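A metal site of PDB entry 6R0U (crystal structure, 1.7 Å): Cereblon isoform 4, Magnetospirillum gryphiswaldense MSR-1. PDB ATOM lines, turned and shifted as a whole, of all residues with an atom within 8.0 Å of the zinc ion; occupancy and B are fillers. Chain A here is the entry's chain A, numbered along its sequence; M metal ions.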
ATOM      1  N   ARG A  24      26.826 -33.103  11.836  1.00  0.00           N
ATOM      2  CA  ARG A  24      26.289 -31.874  11.387  1.00  0.00           C
ATOM      3  C   ARG A  24      24.779 -31.853  11.474  1.00  0.00           C
ATOM      4  O   ARG A  24      24.167 -32.873  11.405  1.00  0.00           O
ATOM      5  CB  ARG A  24      26.685 -31.583   9.922  1.00  0.00           C
ATOM      6  CG  ARG A  24      28.179 -31.336   9.803  1.00  0.00           C
ATOM      7  CD  ARG A  24      28.594 -30.949   8.350  1.00  0.00           C
ATOM      8  NE  ARG A  24      30.035 -30.668   8.325  1.00  0.00           N
ATOM      9  CZ  ARG A  24      30.608 -29.602   8.816  1.00  0.00           C
ATOM     10  NH1 ARG A  24      29.892 -28.540   9.193  1.00  0.00           N
ATOM     11  NH2 ARG A  24      31.941 -29.525   8.807  1.00  0.00           N
ATOM     12  N   CYS A  25      24.182 -30.672  11.553  1.00  0.00           N
ATOM     13  CA  CYS A  25      22.746 -30.544  11.459  1.00  0.00           C
ATOM     14  C   CYS A  25      22.282 -31.115  10.081  1.00  0.00           C
ATOM     15  O   CYS A  25      22.819 -30.699   9.082  1.00  0.00           O
ATOM     16  CB  CYS A  25      22.333 -29.111  11.576  1.00  0.00           C
ATOM     17  SG  CYS A  25      20.501 -28.900  11.339  1.00  0.00           S
ATOM     18  N   ARG A  26      21.321 -32.042  10.100  1.00  0.00           N
ATOM     19  CA  ARG A  26      20.846 -32.676   8.878  1.00  0.00           C
ATOM     20  C   ARG A  26      20.132 -31.673   7.940  1.00  0.00           C
ATOM     21  O   ARG A  26      20.136 -31.888   6.719  1.00  0.00           O
ATOM     22  CB  ARG A  26      19.941 -33.864   9.215  1.00  0.00           C
ATOM     23  CG  ARG A  26      19.309 -34.575   8.105  1.00  0.00           C
ATOM     24  CD  ARG A  26      18.376 -35.641   8.659  1.00  0.00           C
ATOM     25  NE  ARG A  26      17.651 -36.195   7.566  1.00  0.00           N
ATOM     26  CZ  ARG A  26      16.786 -37.220   7.659  1.00  0.00           C
ATOM     27  NH1 ARG A  26      16.602 -37.816   8.808  1.00  0.00           N
ATOM     28  NH2 ARG A  26      16.179 -37.579   6.555  1.00  0.00           N
ATOM     29  N   GLN A  27      19.579 -30.594   8.477  1.00  0.00           N
ATOM     30  CA  GLN A  27      18.852 -29.624   7.690  1.00  0.00           C
ATOM     31  C   GLN A  27      19.671 -28.543   7.062  1.00  0.00           C
ATOM     32  O   GLN A  27      19.318 -28.073   5.980  1.00  0.00           O
ATOM     33  CB  GLN A  27      17.732 -28.998   8.520  1.00  0.00           C
ATOM     34  CG  GLN A  27      16.813 -30.065   9.013  1.00  0.00           C
ATOM     35  CD  GLN A  27      16.092 -30.819   7.887  1.00  0.00           C
ATOM     36  OE1 GLN A  27      15.846 -30.296   6.807  1.00  0.00           O
ATOM     37  NE2 GLN A  27      15.889 -32.080   8.096  1.00  0.00           N
ATOM     38  N   CYS A  28      20.821 -28.190   7.628  1.00  0.00           N
ATOM     39  CA  CYS A  28      21.609 -27.047   7.127  1.00  0.00           C
ATOM     40  C   CYS A  28      23.099 -27.266   7.088  1.00  0.00           C
ATOM     41  O   CYS A  28      23.808 -26.399   6.523  1.00  0.00           O
ATOM     42  CB  CYS A  28      21.285 -25.753   7.854  1.00  0.00           C
ATOM     43  SG  CYS A  28      21.981 -25.827   9.580  1.00  0.00           S
ATOM     44  N   GLY A  29      23.618 -28.318   7.717  1.00  0.00           N
ATOM     45  CA  GLY A  29      25.051 -28.546   7.774  1.00  0.00           C
ATOM     46  C   GLY A  29      25.869 -27.908   8.880  1.00  0.00           C
ATOM     47  O   GLY A  29      27.072 -28.067   8.938  1.00  0.00           O
ATOM     48  N   GLN A  30      25.251 -27.120   9.747  1.00  0.00           N
ATOM     49  CA  GLN A  30      25.960 -26.594  10.917  1.00  0.00           C
ATOM     50  C   GLN A  30      26.738 -27.675  11.679  1.00  0.00           C
ATOM     51  O   GLN A  30      26.173 -28.684  11.959  1.00  0.00           O
ATOM     52  CB  GLN A  30      24.932 -25.946  11.862  1.00  0.00           C
ATOM     53  CG  GLN A  30      25.477 -25.495  13.212  1.00  0.00           C
ATOM     54  CD  GLN A  30      25.924 -24.051  13.182  1.00  0.00           C
ATOM     55  OE1 GLN A  30      26.590 -23.603  12.274  1.00  0.00           O
ATOM     56  NE2 GLN A  30      25.487 -23.287  14.250  1.00  0.00           N
ATOM     57  N   THR A  31      28.001 -27.452  11.988  1.00  0.00           N
ATOM     58  CA  THR A  31      28.777 -28.368  12.811  1.00  0.00           C
ATOM     59  C   THR A  31      28.214 -28.449  14.239  1.00  0.00           C
ATOM     60  O   THR A  31      27.995 -27.374  14.833  1.00  0.00           O
ATOM     61  CB  THR A  31      30.272 -27.905  12.963  1.00  0.00           C
ATOM     62  OG1 THR A  31      30.783 -27.340  11.739  1.00  0.00           O
ATOM     63  CG2 THR A  31      31.063 -29.105  13.474  1.00  0.00           C
ATOM     64  N   ILE A  32      27.911 -29.659  14.711  1.00  0.00           N
ATOM     65  CA  ILE A  32      27.273 -29.854  16.010  1.00  0.00           C
ATOM     66  C   ILE A  32      28.120 -30.674  17.033  1.00  0.00           C
ATOM     67  O   ILE A  32      28.305 -30.233  18.155  1.00  0.00           O
ATOM     68  CB  ILE A  32      25.880 -30.490  15.968  1.00  0.00           C
ATOM     69  CG1 ILE A  32      24.957 -29.711  15.045  1.00  0.00           C
ATOM     70  CG2 ILE A  32      25.283 -30.579  17.376  1.00  0.00           C
ATOM     71  CD1 ILE A  32      24.624 -28.293  15.466  1.00  0.00           C
ATOM     72  N   GLY A  67      27.495 -25.073  18.169  1.00  0.00           N
ATOM     73  CA  GLY A  67      26.589 -24.695  17.069  1.00  0.00           C
ATOM     74  C   GLY A  67      25.114 -24.755  17.403  1.00  0.00           C
ATOM     75  O   GLY A  67      24.311 -24.621  16.519  1.00  0.00           O
ATOM     76  N   LEU A  68      24.772 -24.889  18.644  1.00  0.00           N
ATOM     77  CA  LEU A  68      23.414 -24.980  19.128  1.00  0.00           C
ATOM     78  C   LEU A  68      23.051 -23.652  19.730  1.00  0.00           C
ATOM     79  O   LEU A  68      23.896 -22.801  19.969  1.00  0.00           O
ATOM     80  CB  LEU A  68      23.240 -26.083  20.192  1.00  0.00           C
ATOM     81  CG  LEU A  68      23.503 -27.464  19.736  1.00  0.00           C
ATOM     82  CD1 LEU A  68      23.794 -28.424  20.864  1.00  0.00           C
ATOM     83  CD2 LEU A  68      22.401 -27.996  18.745  1.00  0.00           C
ATOM     84  N   LEU A  90      18.338 -26.091  20.011  1.00  0.00           N
ATOM     85  CA  LEU A  90      18.078 -25.908  18.608  1.00  0.00           C
ATOM     86  C   LEU A  90      19.398 -25.749  17.865  1.00  0.00           C
ATOM     87  O   LEU A  90      20.416 -25.277  18.428  1.00  0.00           O
ATOM     88  CB  LEU A  90      17.270 -24.661  18.402  1.00  0.00           C
ATOM     89  CG  LEU A  90      15.947 -24.534  19.201  1.00  0.00           C
ATOM     90  CD1 LEU A  90      15.261 -23.221  18.791  1.00  0.00           C
ATOM     91  CD2 LEU A  90      15.037 -25.709  18.915  1.00  0.00           C
ATOM     92  N   CYS A  91      19.394 -26.137  16.601  1.00  0.00           N
ATOM     93  CA  CYS A  91      20.465 -25.700  15.678  1.00  0.00           C
ATOM     94  C   CYS A  91      20.565 -24.190  15.705  1.00  0.00           C
ATOM     95  O   CYS A  91      19.573 -23.499  15.477  1.00  0.00           O
ATOM     96  CB  CYS A  91      20.166 -26.159  14.259  1.00  0.00           C
ATOM     97  SG  CYS A  91      21.453 -25.713  13.114  1.00  0.00           S
ATOM     98  N   GLY A  92      21.763 -23.664  15.971  1.00  0.00           N
ATOM     99  CA  GLY A  92      21.974 -22.244  16.104  1.00  0.00           C
ATOM    100  C   GLY A  92      21.915 -21.527  14.761  1.00  0.00           C
ATOM    101  O   GLY A  92      21.745 -20.347  14.707  1.00  0.00           O
ATOM    102  N   GLN A  93      21.999 -22.279  13.682  1.00  0.00           N
ATOM    103  CA  GLN A  93      21.950 -21.756  12.335  1.00  0.00           C
ATOM    104  C   GLN A  93      20.490 -21.718  11.843  1.00  0.00           C
ATOM    105  O   GLN A  93      19.964 -20.677  11.425  1.00  0.00           O
ATOM    106  CB  GLN A  93      22.855 -22.581  11.441  1.00  0.00           C
ATOM    107  CG  GLN A  93      22.983 -22.043  10.072  1.00  0.00           C
ATOM    108  CD  GLN A  93      24.271 -22.465   9.359  1.00  0.00           C
ATOM    109  OE1 GLN A  93      25.184 -21.691   9.317  1.00  0.00           O
ATOM    110  NE2 GLN A  93      24.329 -23.674   8.845  1.00  0.00           N
ATOM    111  N   CYS A  94      19.862 -22.872  11.829  1.00  0.00           N
ATOM    112  CA  CYS A  94      18.551 -23.040  11.148  1.00  0.00           C
ATOM    113  C   CYS A  94      17.314 -23.178  12.059  1.00  0.00           C
ATOM    114  O   CYS A  94      16.210 -23.111  11.576  1.00  0.00           O
ATOM    115  CB  CYS A  94      18.561 -24.140  10.161  1.00  0.00           C
ATOM    116  SG  CYS A  94      18.350 -25.844  10.838  1.00  0.00           S
ATOM    117  N   GLY A  95      17.548 -23.407  13.345  1.00  0.00           N
ATOM    118  CA  GLY A  95      16.492 -23.546  14.312  1.00  0.00           C
ATOM    119  C   GLY A  95      15.897 -24.948  14.433  1.00  0.00           C
ATOM    120  O   GLY A  95      15.002 -25.168  15.262  1.00  0.00           O
ATOM    121  N   SER A  96      16.393 -25.937  13.705  1.00  0.00           N
ATOM    122  CA  SER A  96      15.923 -27.318  13.807  1.00  0.00           C
ATOM    123  C   SER A  96      16.117 -27.790  15.289  1.00  0.00           C
ATOM    124  O   SER A  96      17.122 -27.520  15.928  1.00  0.00           O
ATOM    125  CB  SER A  96      16.689 -28.213  12.893  1.00  0.00           C
ATOM    126  OG  SER A  96      16.334 -29.586  13.080  1.00  0.00           O
ATOM    127  N   HIS A  97      15.083 -28.434  15.856  1.00  0.00           N
ATOM    128  CA  HIS A  97      15.193 -28.942  17.194  1.00  0.00           C
ATOM    129  C   HIS A  97      16.074 -30.203  17.186  1.00  0.00           C
ATOM    130  O   HIS A  97      15.670 -31.240  16.702  1.00  0.00           O
ATOM    131  CB  HIS A  97      13.821 -29.280  17.735  1.00  0.00           C
ATOM    132  CG  HIS A  97      13.903 -29.940  19.097  1.00  0.00           C
ATOM    133  ND1 HIS A  97      12.881 -30.751  19.587  1.00  0.00           N
ATOM    134  CD2 HIS A  97      14.836 -29.828  20.069  1.00  0.00           C
ATOM    135  CE1 HIS A  97      13.260 -31.176  20.787  1.00  0.00           C
ATOM    136  NE2 HIS A  97      14.424 -30.625  21.099  1.00  0.00           N
ATOM    137  N   LEU A  98      17.305 -30.124  17.719  1.00  0.00           N
ATOM    138  CA  LEU A  98      18.255 -31.189  17.623  1.00  0.00           C
ATOM    139  C   LEU A  98      18.361 -32.051  18.883  1.00  0.00           C
ATOM    140  O   LEU A  98      18.858 -33.144  18.837  1.00  0.00           O
ATOM    141  CB  LEU A  98      19.656 -30.642  17.253  1.00  0.00           C
ATOM    142  CG  LEU A  98      19.786 -29.964  15.868  1.00  0.00           C
ATOM    143  CD1 LEU A  98      21.255 -29.708  15.493  1.00  0.00           C
ATOM    144  CD2 LEU A  98      19.223 -30.825  14.737  1.00  0.00           C
ATOM    145  N   ARG A 118      18.340 -36.545  13.385  1.00  0.00           N
ATOM    146  CA  ARG A 118      18.385 -35.160  13.000  1.00  0.00           C
ATOM    147  C   ARG A 118      19.789 -34.634  12.730  1.00  0.00           C
ATOM    148  O   ARG A 118      19.980 -33.450  12.452  1.00  0.00           O
ATOM    149  CB  ARG A 118      17.716 -34.324  14.090  1.00  0.00           C
ATOM    150  CG  ARG A 118      16.233 -34.792  14.173  1.00  0.00           C
ATOM    151  CD  ARG A 118      15.364 -33.907  14.986  1.00  0.00           C
ATOM    152  NE  ARG A 118      14.049 -34.537  15.148  1.00  0.00           N
ATOM    153  CZ  ARG A 118      13.008 -33.982  15.775  1.00  0.00           C
ATOM    154  NH1 ARG A 118      13.132 -32.774  16.345  1.00  0.00           N
ATOM    155  NH2 ARG A 118      11.852 -34.656  15.888  1.00  0.00           N
HETATM  156 ZN    ZN M   1      20.517 -26.615  11.180  1.00  0.00          ZN
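Four residues have an atom within 4 Å of the zinc ion: Cys 25, Cys 28, Cys 91 and Cys 94.
The side-chain sulfur (SG) of Cys 28 sits close to the side-chain amide nitrogen (NE2) of Gln 93 (3.3 Å). N of Cys 25 lies within hydrogen-bond range of O of Gln 30 (2.8 Å). N of Ser 96 lies close to SG of Cys 94 (3.5 Å). SG of Cys 25 sits close to N of Gln 27, 3.5 Å away. The backbone carbonyl oxygen (O) of Ser 96 sits at hydrogen-bond distance from the backbone NH (N) of Cys 91, 2.7 Å away. The side-chain sulfur (SG) of Cys 28 lies close to the backbone NH (N) of Gln 30 (3.5 Å). The side-chain sulfur (SG) of Cys 91 lies close to the backbone NH (N) of Gln 93 (3.5 Å).
SG of Cys 25 binds the zinc ion (2.3 Å). SG of Cys 28 is bound to the zinc ion (2.3 Å). SG of Cys 94 is bound to the zinc ion, 2.3 Å away. The zinc ion is bound by SG of Cys 91, at 2.3 Å. The zinc ion has four donor atoms within binding distance.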
